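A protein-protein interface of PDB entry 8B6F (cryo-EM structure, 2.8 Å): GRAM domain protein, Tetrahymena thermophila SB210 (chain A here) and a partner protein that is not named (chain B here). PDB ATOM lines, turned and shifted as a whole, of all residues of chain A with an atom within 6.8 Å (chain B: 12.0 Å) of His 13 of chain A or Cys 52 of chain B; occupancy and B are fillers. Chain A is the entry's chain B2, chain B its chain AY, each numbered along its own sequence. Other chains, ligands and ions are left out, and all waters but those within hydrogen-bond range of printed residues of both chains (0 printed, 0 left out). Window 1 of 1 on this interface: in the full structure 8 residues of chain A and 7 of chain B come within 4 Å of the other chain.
Of the 18 printed residues of chain B, 6 touch a printed residue of chain A. Printed residues of chain B that touch a printed residue of chain A: Ile 50, Tyr 51, Cys 52, Asp 53, Ile 54 and Leu 57. Hydrophobic or aromatic side chains of chain B that line the printed part of chain A: Ile 50, Tyr 51, Ile 54 and Leu 57. Printed residues of chain A that touch a printed residue of chain B: Ser 4, Tyr 6, Ser 7, Leu 8, His 13, His 47 and Arg 49. Hydrophobic or aromatic side chains of chain A that line the printed part of chain B: Tyr 6, Leu 8, His 13 and His 47. Among the printed residues, 13 pairs touch across the chains. Among the printed residues, no Asp or Glu carboxylate lies within 4 Å of a Lys or Arg side-chain nitrogen of the other chain.
Ser 4 of chain A touches just one residue of chain B: Ile 54. Printed residues of chain B within 4 Å of Tyr 6 of chain A: Cys 52 and Ile 54. Ser 7 of chain A touches just these residues of chain B: Cys 52 (3.6 Å) and Ile 54 (3.0 Å). Of the printed residues of chain B, Leu 8 of chain A touches Cys 52, Asp 53 and Leu 57. No residue of chain B comes within 4 Å of Gly 11 of chain A. No residue of chain B comes within 4 Å of Val 12 of chain A. Of chain B, only Tyr 51 and Cys 52 come within 4 Å of His 13 of chain A. No residue of chain B comes within 4 Å of Cys 15 of chain A. No residue of chain B comes within 4 Å of Leu 16 of chain A. Cys 46 of chain A touches none of the printed residues of chain B. His 47 of chain A touches just one residue of chain B: Tyr 51 (3.4 Å). Ile 5 of chain B touches none of the printed residues of chain A. Of the printed residues of chain A, Ile 50 of chain B touches Arg 49 (3.5 Å). Of the printed residues of chain A, Cys 52 of chain B touches Tyr 6, Ser 7, Leu 8 and His 13. Printed residues of chain A within 4 Å of Asp 53 of chain B: Leu 8.
Among the printed residues, pairs that only touch across the chains: Ser 7 of chain A with Ile 54 of chain B (3.0 Å), Ser 4 of chain A with Ile 54 of chain B (3.2 Å), His 47 of chain A with Tyr 51 of chain B (3.4 Å), Leu 8 of chain A with Leu 57 of chain B (3.5 Å), Arg 49 of chain A with Ile 50 of chain B (3.5 Å), Tyr 6 of chain A with Cys 52 of chain B (3.5 Å), Ser 7 of chain A with Cys 52 of chain B (3.6 Å), Tyr 6 of chain A with Ile 54 of chain B (3.7 Å), Arg 49 of chain A with Tyr 51 of chain B (3.8 Å) and Leu 8 of chain A with Asp 53 of chain B (3.9 Å).
O of Ile 54 of chain B sits at hydrogen-bond distance from OG of Ser 58 of chain B (3.0 Å). The backbone carbonyl oxygen (O) of Gly 48 of chain B is in hydrogen-bond range of the backbone NH (N) of Asp 53 of chain B, at 3.1 Å. O of His 47 of chain A lies within hydrogen-bond range of NH2 of Arg 49 of chain A, at 3.4 Å. OG of Ser 7 of chain A sits at hydrogen-bond distance from N of Gly 11 of chain A (2.6 Å). A ring nitrogen (ND1) of His 13 of chain A sits at hydrogen-bond distance from the side-chain hydroxyl of Tyr 3 of chain A, at 3.0 Å. OG of Ser 7 of chain A lies within hydrogen-bond range of OD1 of Asn 9 of chain A, at 2.5 Å.
O of Tyr 51 of chain B lies within hydrogen-bond range of NE2 of His 13 of chain A (2.9 Å). The backbone carbonyl oxygen of Cys 52 of chain B lies close to a ring nitrogen (NE2) of His 13 of chain A, at 3.3 Å. SG of Cys 52 of chain B sits at hydrogen-bond distance from N of Leu 8 of chain A (3.7 Å).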
ATOM      1  N   TYR A   3     -13.957  26.756  16.215  1.00  0.00           N
ATOM      2  CA  TYR A   3     -15.332  27.102  16.568  1.00  0.00           C
ATOM      3  C   TYR A   3     -16.195  25.866  16.343  1.00  0.00           C
ATOM      4  O   TYR A   3     -16.654  25.607  15.229  1.00  0.00           O
ATOM      5  CB  TYR A   3     -15.825  28.284  15.742  1.00  0.00           C
ATOM      6  CG  TYR A   3     -17.241  28.689  16.063  1.00  0.00           C
ATOM      7  CD1 TYR A   3     -17.511  29.545  17.121  1.00  0.00           C
ATOM      8  CD2 TYR A   3     -18.307  28.214  15.312  1.00  0.00           C
ATOM      9  CE1 TYR A   3     -18.801  29.919  17.423  1.00  0.00           C
ATOM     10  CE2 TYR A   3     -19.604  28.584  15.608  1.00  0.00           C
ATOM     11  CZ  TYR A   3     -19.842  29.433  16.668  1.00  0.00           C
ATOM     12  OH  TYR A   3     -21.124  29.808  16.971  1.00  0.00           O
ATOM     13  N   SER A   4     -16.412  25.095  17.409  1.00  0.00           N
ATOM     14  CA  SER A   4     -17.186  23.864  17.289  1.00  0.00           C
ATOM     15  C   SER A   4     -18.631  24.149  16.899  1.00  0.00           C
ATOM     16  O   SER A   4     -19.225  23.410  16.107  1.00  0.00           O
ATOM     17  CB  SER A   4     -17.134  23.091  18.601  1.00  0.00           C
ATOM     18  OG  SER A   4     -17.706  23.862  19.634  1.00  0.00           O
ATOM     19  N   GLY A   5     -19.214  25.209  17.448  1.00  0.00           N
ATOM     20  CA  GLY A   5     -20.596  25.540  17.176  1.00  0.00           C
ATOM     21  C   GLY A   5     -21.613  24.833  18.044  1.00  0.00           C
ATOM     22  O   GLY A   5     -22.806  24.876  17.724  1.00  0.00           O
ATOM     23  N   TYR A   6     -21.187  24.186  19.123  1.00  0.00           N
ATOM     24  CA  TYR A   6     -22.087  23.516  20.048  1.00  0.00           C
ATOM     25  C   TYR A   6     -22.323  24.375  21.285  1.00  0.00           C
ATOM     26  O   TYR A   6     -21.535  25.262  21.618  1.00  0.00           O
ATOM     27  CB  TYR A   6     -21.522  22.160  20.470  1.00  0.00           C
ATOM     28  CG  TYR A   6     -21.449  21.142  19.361  1.00  0.00           C
ATOM     29  CD1 TYR A   6     -22.575  20.431  18.971  1.00  0.00           C
ATOM     30  CD2 TYR A   6     -20.251  20.877  18.715  1.00  0.00           C
ATOM     31  CE1 TYR A   6     -22.511  19.493  17.961  1.00  0.00           C
ATOM     32  CE2 TYR A   6     -20.177  19.942  17.705  1.00  0.00           C
ATOM     33  CZ  TYR A   6     -21.309  19.253  17.332  1.00  0.00           C
ATOM     34  OH  TYR A   6     -21.237  18.320  16.327  1.00  0.00           O
ATOM     35  N   SER A   7     -23.430  24.095  21.969  1.00  0.00           N
ATOM     36  CA  SER A   7     -23.744  24.750  23.227  1.00  0.00           C
ATOM     37  C   SER A   7     -23.210  23.899  24.378  1.00  0.00           C
ATOM     38  O   SER A   7     -22.493  22.918  24.169  1.00  0.00           O
ATOM     39  CB  SER A   7     -25.247  24.994  23.341  1.00  0.00           C
ATOM     40  OG  SER A   7     -25.963  23.772  23.373  1.00  0.00           O
ATOM     41  N   LEU A   8     -23.553  24.266  25.610  1.00  0.00           N
ATOM     42  CA  LEU A   8     -23.093  23.526  26.777  1.00  0.00           C
ATOM     43  C   LEU A   8     -23.968  22.324  27.105  1.00  0.00           C
ATOM     44  O   LEU A   8     -23.654  21.593  28.049  1.00  0.00           O
ATOM     45  CB  LEU A   8     -23.022  24.454  27.993  1.00  0.00           C
ATOM     46  CG  LEU A   8     -22.081  25.659  27.875  1.00  0.00           C
ATOM     47  CD1 LEU A   8     -21.940  26.370  29.211  1.00  0.00           C
ATOM     48  CD2 LEU A   8     -20.728  25.273  27.315  1.00  0.00           C
ATOM     49  N   ASN A   9     -25.053  22.107  26.362  1.00  0.00           N
ATOM     50  CA  ASN A   9     -25.885  20.919  26.516  1.00  0.00           C
ATOM     51  C   ASN A   9     -25.952  20.114  25.225  1.00  0.00           C
ATOM     52  O   ASN A   9     -26.906  19.358  25.017  1.00  0.00           O
ATOM     53  CB  ASN A   9     -27.293  21.301  26.975  1.00  0.00           C
ATOM     54  CG  ASN A   9     -28.031  22.137  25.954  1.00  0.00           C
ATOM     55  OD1 ASN A   9     -27.420  22.838  25.149  1.00  0.00           O
ATOM     56  ND2 ASN A   9     -29.355  22.070  25.983  1.00  0.00           N
ATOM     57  N   GLY A  11     -26.398  21.396  22.287  1.00  0.00           N
ATOM     58  CA  GLY A  11     -27.185  22.118  21.307  1.00  0.00           C
ATOM     59  C   GLY A  11     -26.317  22.885  20.335  1.00  0.00           C
ATOM     60  O   GLY A  11     -25.202  22.473  19.997  1.00  0.00           O
ATOM     61  N   VAL A  12     -26.831  24.023  19.878  1.00  0.00           N
ATOM     62  CA  VAL A  12     -26.147  24.872  18.909  1.00  0.00           C
ATOM     63  C   VAL A  12     -25.691  26.143  19.605  1.00  0.00           C
ATOM     64  O   VAL A  12     -26.450  26.756  20.365  1.00  0.00           O
ATOM     65  CB  VAL A  12     -27.048  25.186  17.702  1.00  0.00           C
ATOM     66  CG1 VAL A  12     -26.541  26.399  16.932  1.00  0.00           C
ATOM     67  CG2 VAL A  12     -27.108  23.985  16.784  1.00  0.00           C
ATOM     68  N   HIS A  13     -24.449  26.534  19.342  1.00  0.00           N
ATOM     69  CA  HIS A  13     -23.898  27.735  19.941  1.00  0.00           C
ATOM     70  C   HIS A  13     -24.724  28.945  19.512  1.00  0.00           C
ATOM     71  O   HIS A  13     -25.084  29.063  18.335  1.00  0.00           O
ATOM     72  CB  HIS A  13     -22.439  27.908  19.515  1.00  0.00           C
ATOM     73  CG  HIS A  13     -21.674  28.880  20.354  1.00  0.00           C
ATOM     74  ND1 HIS A  13     -21.411  30.169  19.944  1.00  0.00           N
ATOM     75  CD2 HIS A  13     -21.111  28.753  21.578  1.00  0.00           C
ATOM     76  CE1 HIS A  13     -20.722  30.796  20.880  1.00  0.00           C
ATOM     77  NE2 HIS A  13     -20.526  29.959  21.882  1.00  0.00           N
ATOM     78  N   PRO A  14     -25.046  29.862  20.429  1.00  0.00           N
ATOM     79  CA  PRO A  14     -25.886  31.008  20.047  1.00  0.00           C
ATOM     80  C   PRO A  14     -25.268  31.899  18.984  1.00  0.00           C
ATOM     81  O   PRO A  14     -26.008  32.603  18.288  1.00  0.00           O
ATOM     82  CB  PRO A  14     -26.076  31.760  21.372  1.00  0.00           C
ATOM     83  CG  PRO A  14     -24.928  31.342  22.215  1.00  0.00           C
ATOM     84  CD  PRO A  14     -24.653  29.921  21.848  1.00  0.00           C
ATOM     85  N   CYS A  15     -23.946  31.898  18.835  1.00  0.00           N
ATOM     86  CA  CYS A  15     -23.275  32.731  17.846  1.00  0.00           C
ATOM     87  C   CYS A  15     -23.213  32.088  16.468  1.00  0.00           C
ATOM     88  O   CYS A  15     -22.691  32.710  15.538  1.00  0.00           O
ATOM     89  CB  CYS A  15     -21.851  33.062  18.308  1.00  0.00           C
ATOM     90  SG  CYS A  15     -21.763  33.944  19.875  1.00  0.00           S
ATOM     91  N   LEU A  16     -23.722  30.866  16.311  1.00  0.00           N
ATOM     92  CA  LEU A  16     -23.540  30.156  15.048  1.00  0.00           C
ATOM     93  C   LEU A  16     -24.111  30.910  13.856  1.00  0.00           C
ATOM     94  O   LEU A  16     -23.428  30.967  12.819  1.00  0.00           O
ATOM     95  CB  LEU A  16     -24.154  28.754  15.145  1.00  0.00           C
ATOM     96  CG  LEU A  16     -24.018  27.882  13.893  1.00  0.00           C
ATOM     97  CD1 LEU A  16     -22.555  27.626  13.567  1.00  0.00           C
ATOM     98  CD2 LEU A  16     -24.758  26.569  14.063  1.00  0.00           C
ATOM     99  N   PRO A  17     -25.310  31.490  13.912  1.00  0.00           N
ATOM    100  CA  PRO A  17     -25.784  32.241  12.739  1.00  0.00           C
ATOM    101  C   PRO A  17     -24.859  33.384  12.362  1.00  0.00           C
ATOM    102  O   PRO A  17     -24.527  33.546  11.182  1.00  0.00           O
ATOM    103  CB  PRO A  17     -27.169  32.730  13.181  1.00  0.00           C
ATOM    104  CG  PRO A  17     -27.586  31.784  14.244  1.00  0.00           C
ATOM    105  CD  PRO A  17     -26.333  31.421  14.968  1.00  0.00           C
ATOM    106  N   TYR A  43     -21.028  39.419  14.822  1.00  0.00           N
ATOM    107  CA  TYR A  43     -20.481  38.236  15.477  1.00  0.00           C
ATOM    108  C   TYR A  43     -19.734  38.615  16.748  1.00  0.00           C
ATOM    109  O   TYR A  43     -19.903  37.982  17.796  1.00  0.00           O
ATOM    110  CB  TYR A  43     -19.561  37.482  14.517  1.00  0.00           C
ATOM    111  CG  TYR A  43     -18.688  36.456  15.204  1.00  0.00           C
ATOM    112  CD1 TYR A  43     -19.207  35.239  15.621  1.00  0.00           C
ATOM    113  CD2 TYR A  43     -17.344  36.710  15.436  1.00  0.00           C
ATOM    114  CE1 TYR A  43     -18.412  34.305  16.250  1.00  0.00           C
ATOM    115  CE2 TYR A  43     -16.541  35.783  16.063  1.00  0.00           C
ATOM    116  CZ  TYR A  43     -17.080  34.583  16.467  1.00  0.00           C
ATOM    117  OH  TYR A  43     -16.281  33.657  17.092  1.00  0.00           O
ATOM    118  N   CYS A  46     -22.277  39.463  19.433  1.00  0.00           N
ATOM    119  CA  CYS A  46     -22.883  38.274  20.017  1.00  0.00           C
ATOM    120  C   CYS A  46     -21.901  37.503  20.883  1.00  0.00           C
ATOM    121  O   CYS A  46     -22.327  36.760  21.773  1.00  0.00           O
ATOM    122  CB  CYS A  46     -23.420  37.366  18.910  1.00  0.00           C
ATOM    123  SG  CYS A  46     -24.492  36.043  19.500  1.00  0.00           S
ATOM    124  N   HIS A  47     -20.597  37.661  20.648  1.00  0.00           N
ATOM    125  CA  HIS A  47     -19.584  36.940  21.407  1.00  0.00           C
ATOM    126  C   HIS A  47     -19.198  37.660  22.695  1.00  0.00           C
ATOM    127  O   HIS A  47     -19.127  37.038  23.757  1.00  0.00           O
ATOM    128  CB  HIS A  47     -18.345  36.720  20.536  1.00  0.00           C
ATOM    129  CG  HIS A  47     -17.252  35.966  21.224  1.00  0.00           C
ATOM    130  ND1 HIS A  47     -17.408  34.670  21.670  1.00  0.00           N
ATOM    131  CD2 HIS A  47     -15.988  36.323  21.546  1.00  0.00           C
ATOM    132  CE1 HIS A  47     -16.286  34.264  22.235  1.00  0.00           C
ATOM    133  NE2 HIS A  47     -15.408  35.247  22.173  1.00  0.00           N
ATOM    134  N   ARG A  49     -20.538  40.967  23.849  1.00  0.00           N
ATOM    135  CA  ARG A  49     -21.630  41.696  24.490  1.00  0.00           C
ATOM    136  C   ARG A  49     -21.158  43.028  25.063  1.00  0.00           C
ATOM    137  O   ARG A  49     -21.657  43.480  26.095  1.00  0.00           O
ATOM    138  CB  ARG A  49     -22.303  40.852  25.577  1.00  0.00           C
ATOM    139  CG  ARG A  49     -22.985  39.606  25.037  1.00  0.00           C
ATOM    140  CD  ARG A  49     -22.944  38.462  26.032  1.00  0.00           C
ATOM    141  NE  ARG A  49     -21.616  37.869  26.129  1.00  0.00           N
ATOM    142  CZ  ARG A  49     -21.307  36.852  26.921  1.00  0.00           C
ATOM    143  NH1 ARG A  49     -22.208  36.289  27.708  1.00  0.00           N
ATOM    144  NH2 ARG A  49     -20.062  36.389  26.924  1.00  0.00           N
ATOM    145  N   ILE B   5     -13.635  37.023  36.675  1.00  0.00           N
ATOM    146  CA  ILE B   5     -12.667  37.059  35.582  1.00  0.00           C
ATOM    147  C   ILE B   5     -11.377  37.714  36.052  1.00  0.00           C
ATOM    148  O   ILE B   5     -10.282  37.163  35.891  1.00  0.00           O
ATOM    149  CB  ILE B   5     -13.255  37.791  34.361  1.00  0.00           C
ATOM    150  CG1 ILE B   5     -14.392  36.992  33.716  1.00  0.00           C
ATOM    151  CG2 ILE B   5     -12.178  38.055  33.315  1.00  0.00           C
ATOM    152  CD1 ILE B   5     -15.705  37.033  34.473  1.00  0.00           C
ATOM    153  N   LEU B  43      -9.695  28.662  35.564  1.00  0.00           N
ATOM    154  CA  LEU B  43      -9.873  29.787  34.651  1.00  0.00           C
ATOM    155  C   LEU B  43     -10.473  29.336  33.327  1.00  0.00           C
ATOM    156  O   LEU B  43     -11.359  30.002  32.779  1.00  0.00           O
ATOM    157  CB  LEU B  43      -8.534  30.493  34.419  1.00  0.00           C
ATOM    158  CG  LEU B  43      -8.552  31.679  33.448  1.00  0.00           C
ATOM    159  CD1 LEU B  43      -9.476  32.778  33.948  1.00  0.00           C
ATOM    160  CD2 LEU B  43      -7.150  32.217  33.236  1.00  0.00           C
ATOM    161  N   SER B  44     -10.003  28.208  32.794  1.00  0.00           N
ATOM    162  CA  SER B  44     -10.555  27.699  31.544  1.00  0.00           C
ATOM    163  C   SER B  44     -12.027  27.342  31.697  1.00  0.00           C
ATOM    164  O   SER B  44     -12.837  27.628  30.808  1.00  0.00           O
ATOM    165  CB  SER B  44      -9.753  26.485  31.076  1.00  0.00           C
ATOM    166  OG  SER B  44      -9.774  25.454  32.045  1.00  0.00           O
ATOM    167  N   LEU B  45     -12.394  26.717  32.815  1.00  0.00           N
ATOM    168  CA  LEU B  45     -13.801  26.404  33.049  1.00  0.00           C
ATOM    169  C   LEU B  45     -14.636  27.673  33.141  1.00  0.00           C
ATOM    170  O   LEU B  45     -15.754  27.727  32.616  1.00  0.00           O
ATOM    171  CB  LEU B  45     -13.950  25.571  34.322  1.00  0.00           C
ATOM    172  CG  LEU B  45     -13.492  24.112  34.250  1.00  0.00           C
ATOM    173  CD1 LEU B  45     -13.684  23.441  35.594  1.00  0.00           C
ATOM    174  CD2 LEU B  45     -14.231  23.342  33.167  1.00  0.00           C
ATOM    175  N   LEU B  46     -14.119  28.701  33.814  1.00  0.00           N
ATOM    176  CA  LEU B  46     -14.857  29.954  33.926  1.00  0.00           C
ATOM    177  C   LEU B  46     -15.112  30.560  32.551  1.00  0.00           C
ATOM    178  O   LEU B  46     -16.239  30.955  32.233  1.00  0.00           O
ATOM    179  CB  LEU B  46     -14.082  30.929  34.814  1.00  0.00           C
ATOM    180  CG  LEU B  46     -14.626  32.353  34.925  1.00  0.00           C
ATOM    181  CD1 LEU B  46     -16.027  32.350  35.496  1.00  0.00           C
ATOM    182  CD2 LEU B  46     -13.705  33.206  35.776  1.00  0.00           C
ATOM    183  N   PHE B  47     -14.073  30.644  31.719  1.00  0.00           N
ATOM    184  CA  PHE B  47     -14.240  31.226  30.392  1.00  0.00           C
ATOM    185  C   PHE B  47     -15.145  30.365  29.521  1.00  0.00           C
ATOM    186  O   PHE B  47     -15.935  30.892  28.729  1.00  0.00           O
ATOM    187  CB  PHE B  47     -12.880  31.423  29.721  1.00  0.00           C
ATOM    188  CG  PHE B  47     -12.181  32.693  30.122  1.00  0.00           C
ATOM    189  CD1 PHE B  47     -12.551  33.382  31.266  1.00  0.00           C
ATOM    190  CD2 PHE B  47     -11.162  33.205  29.340  1.00  0.00           C
ATOM    191  CE1 PHE B  47     -11.910  34.549  31.624  1.00  0.00           C
ATOM    192  CE2 PHE B  47     -10.518  34.372  29.694  1.00  0.00           C
ATOM    193  CZ  PHE B  47     -10.892  35.044  30.837  1.00  0.00           C
ATOM    194  N   GLY B  48     -15.046  29.043  29.648  1.00  0.00           N
ATOM    195  CA  GLY B  48     -15.938  28.174  28.900  1.00  0.00           C
ATOM    196  C   GLY B  48     -17.393  28.385  29.260  1.00  0.00           C
ATOM    197  O   GLY B  48     -18.263  28.417  28.387  1.00  0.00           O
ATOM    198  N   ALA B  49     -17.683  28.528  30.554  1.00  0.00           N
ATOM    199  CA  ALA B  49     -19.049  28.821  30.972  1.00  0.00           C
ATOM    200  C   ALA B  49     -19.508  30.170  30.437  1.00  0.00           C
ATOM    201  O   ALA B  49     -20.655  30.317  30.001  1.00  0.00           O
ATOM    202  CB  ALA B  49     -19.147  28.789  32.496  1.00  0.00           C
ATOM    203  N   ILE B  50     -18.628  31.173  30.475  1.00  0.00           N
ATOM    204  CA  ILE B  50     -19.007  32.517  30.048  1.00  0.00           C
ATOM    205  C   ILE B  50     -19.334  32.535  28.561  1.00  0.00           C
ATOM    206  O   ILE B  50     -20.344  33.107  28.137  1.00  0.00           O
ATOM    207  CB  ILE B  50     -17.882  33.513  30.388  1.00  0.00           C
ATOM    208  CG1 ILE B  50     -17.815  33.729  31.898  1.00  0.00           C
ATOM    209  CG2 ILE B  50     -18.094  34.843  29.672  1.00  0.00           C
ATOM    210  CD1 ILE B  50     -16.593  34.479  32.351  1.00  0.00           C
ATOM    211  N   TYR B  51     -18.480  31.917  27.745  1.00  0.00           N
ATOM    212  CA  TYR B  51     -18.586  32.021  26.297  1.00  0.00           C
ATOM    213  C   TYR B  51     -19.276  30.822  25.658  1.00  0.00           C
ATOM    214  O   TYR B  51     -19.338  30.743  24.429  1.00  0.00           O
ATOM    215  CB  TYR B  51     -17.196  32.203  25.687  1.00  0.00           C
ATOM    216  CG  TYR B  51     -16.532  33.504  26.072  1.00  0.00           C
ATOM    217  CD1 TYR B  51     -16.934  34.704  25.505  1.00  0.00           C
ATOM    218  CD2 TYR B  51     -15.495  33.529  26.996  1.00  0.00           C
ATOM    219  CE1 TYR B  51     -16.329  35.894  25.852  1.00  0.00           C
ATOM    220  CE2 TYR B  51     -14.884  34.715  27.350  1.00  0.00           C
ATOM    221  CZ  TYR B  51     -15.306  35.893  26.775  1.00  0.00           C
ATOM    222  OH  TYR B  51     -14.700  37.077  27.121  1.00  0.00           O
ATOM    223  N   CYS B  52     -19.799  29.894  26.457  1.00  0.00           N
ATOM    224  CA  CYS B  52     -20.502  28.726  25.931  1.00  0.00           C
ATOM    225  C   CYS B  52     -19.598  27.910  25.008  1.00  0.00           C
ATOM    226  O   CYS B  52     -20.030  27.419  23.965  1.00  0.00           O
ATOM    227  CB  CYS B  52     -21.778  29.148  25.201  1.00  0.00           C
ATOM    228  SG  CYS B  52     -22.941  27.814  24.886  1.00  0.00           S
ATOM    229  N   ASP B  53     -18.336  27.758  25.396  1.00  0.00           N
ATOM    230  CA  ASP B  53     -17.321  27.117  24.565  1.00  0.00           C
ATOM    231  C   ASP B  53     -17.030  25.723  25.109  1.00  0.00           C
ATOM    232  O   ASP B  53     -16.390  25.581  26.155  1.00  0.00           O
ATOM    233  CB  ASP B  53     -16.053  27.966  24.518  1.00  0.00           C
ATOM    234  CG  ASP B  53     -15.087  27.513  23.441  1.00  0.00           C
ATOM    235  OD1 ASP B  53     -15.356  26.478  22.797  1.00  0.00           O
ATOM    236  OD2 ASP B  53     -14.063  28.194  23.234  1.00  0.00           O
ATOM    237  N   ILE B  54     -17.496  24.695  24.395  1.00  0.00           N
ATOM    238  CA  ILE B  54     -17.251  23.320  24.828  1.00  0.00           C
ATOM    239  C   ILE B  54     -15.763  23.003  24.796  1.00  0.00           C
ATOM    240  O   ILE B  54     -15.282  22.169  25.573  1.00  0.00           O
ATOM    241  CB  ILE B  54     -18.056  22.317  23.979  1.00  0.00           C
ATOM    242  CG1 ILE B  54     -17.649  22.398  22.512  1.00  0.00           C
ATOM    243  CG2 ILE B  54     -19.541  22.599  24.108  1.00  0.00           C
ATOM    244  CD1 ILE B  54     -18.121  21.225  21.681  1.00  0.00           C
ATOM    245  N   THR B  55     -15.012  23.644  23.900  1.00  0.00           N
ATOM    246  CA  THR B  55     -13.568  23.438  23.866  1.00  0.00           C
ATOM    247  C   THR B  55     -12.921  23.932  25.153  1.00  0.00           C
ATOM    248  O   THR B  55     -12.065  23.252  25.731  1.00  0.00           O
ATOM    249  CB  THR B  55     -12.962  24.148  22.654  1.00  0.00           C
ATOM    250  OG1 THR B  55     -13.605  23.694  21.455  1.00  0.00           O
ATOM    251  CG2 THR B  55     -11.470  23.861  22.556  1.00  0.00           C
ATOM    252  N   LEU B  56     -13.310  25.121  25.616  1.00  0.00           N
ATOM    253  CA  LEU B  56     -12.772  25.632  26.875  1.00  0.00           C
ATOM    254  C   LEU B  56     -13.169  24.746  28.049  1.00  0.00           C
ATOM    255  O   LEU B  56     -12.355  24.485  28.940  1.00  0.00           O
ATOM    256  CB  LEU B  56     -13.241  27.068  27.099  1.00  0.00           C
ATOM    257  CG  LEU B  56     -12.574  28.135  26.226  1.00  0.00           C
ATOM    258  CD1 LEU B  56     -13.222  29.485  26.445  1.00  0.00           C
ATOM    259  CD2 LEU B  56     -11.086  28.219  26.510  1.00  0.00           C
ATOM    260  N   LEU B  57     -14.415  24.269  28.067  1.00  0.00           N
ATOM    261  CA  LEU B  57     -14.839  23.363  29.130  1.00  0.00           C
ATOM    262  C   LEU B  57     -14.035  22.073  29.094  1.00  0.00           C
ATOM    263  O   LEU B  57     -13.640  21.547  30.141  1.00  0.00           O
ATOM    264  CB  LEU B  57     -16.330  23.049  29.029  1.00  0.00           C
ATOM    265  CG  LEU B  57     -17.322  24.114  29.495  1.00  0.00           C
ATOM    266  CD1 LEU B  57     -18.705  23.511  29.493  1.00  0.00           C
ATOM    267  CD2 LEU B  57     -16.988  24.669  30.870  1.00  0.00           C
ATOM    268  N   SER B  58     -13.786  21.548  27.899  1.00  0.00           N
ATOM    269  CA  SER B  58     -13.100  20.276  27.765  1.00  0.00           C
ATOM    270  C   SER B  58     -11.608  20.385  28.018  1.00  0.00           C
ATOM    271  O   SER B  58     -10.956  19.361  28.250  1.00  0.00           O
ATOM    272  CB  SER B  58     -13.281  19.781  26.343  1.00  0.00           C
ATOM    273  OG  SER B  58     -12.661  20.743  25.498  1.00  0.00           O
ATOM    274  N   ILE B  59     -11.050  21.596  27.974  1.00  0.00           N
ATOM    275  CA  ILE B  59      -9.646  21.793  28.308  1.00  0.00           C
ATOM    276  C   ILE B  59      -9.354  21.287  29.713  1.00  0.00           C
ATOM    277  O   ILE B  59      -8.194  21.038  30.056  1.00  0.00           O
ATOM    278  CB  ILE B  59      -9.270  23.280  28.135  1.00  0.00           C
ATOM    279  CG1 ILE B  59      -8.961  23.563  26.664  1.00  0.00           C
ATOM    280  CG2 ILE B  59      -8.081  23.656  29.010  1.00  0.00           C
ATOM    281  CD1 ILE B  59      -8.740  25.026  26.344  1.00  0.00           C
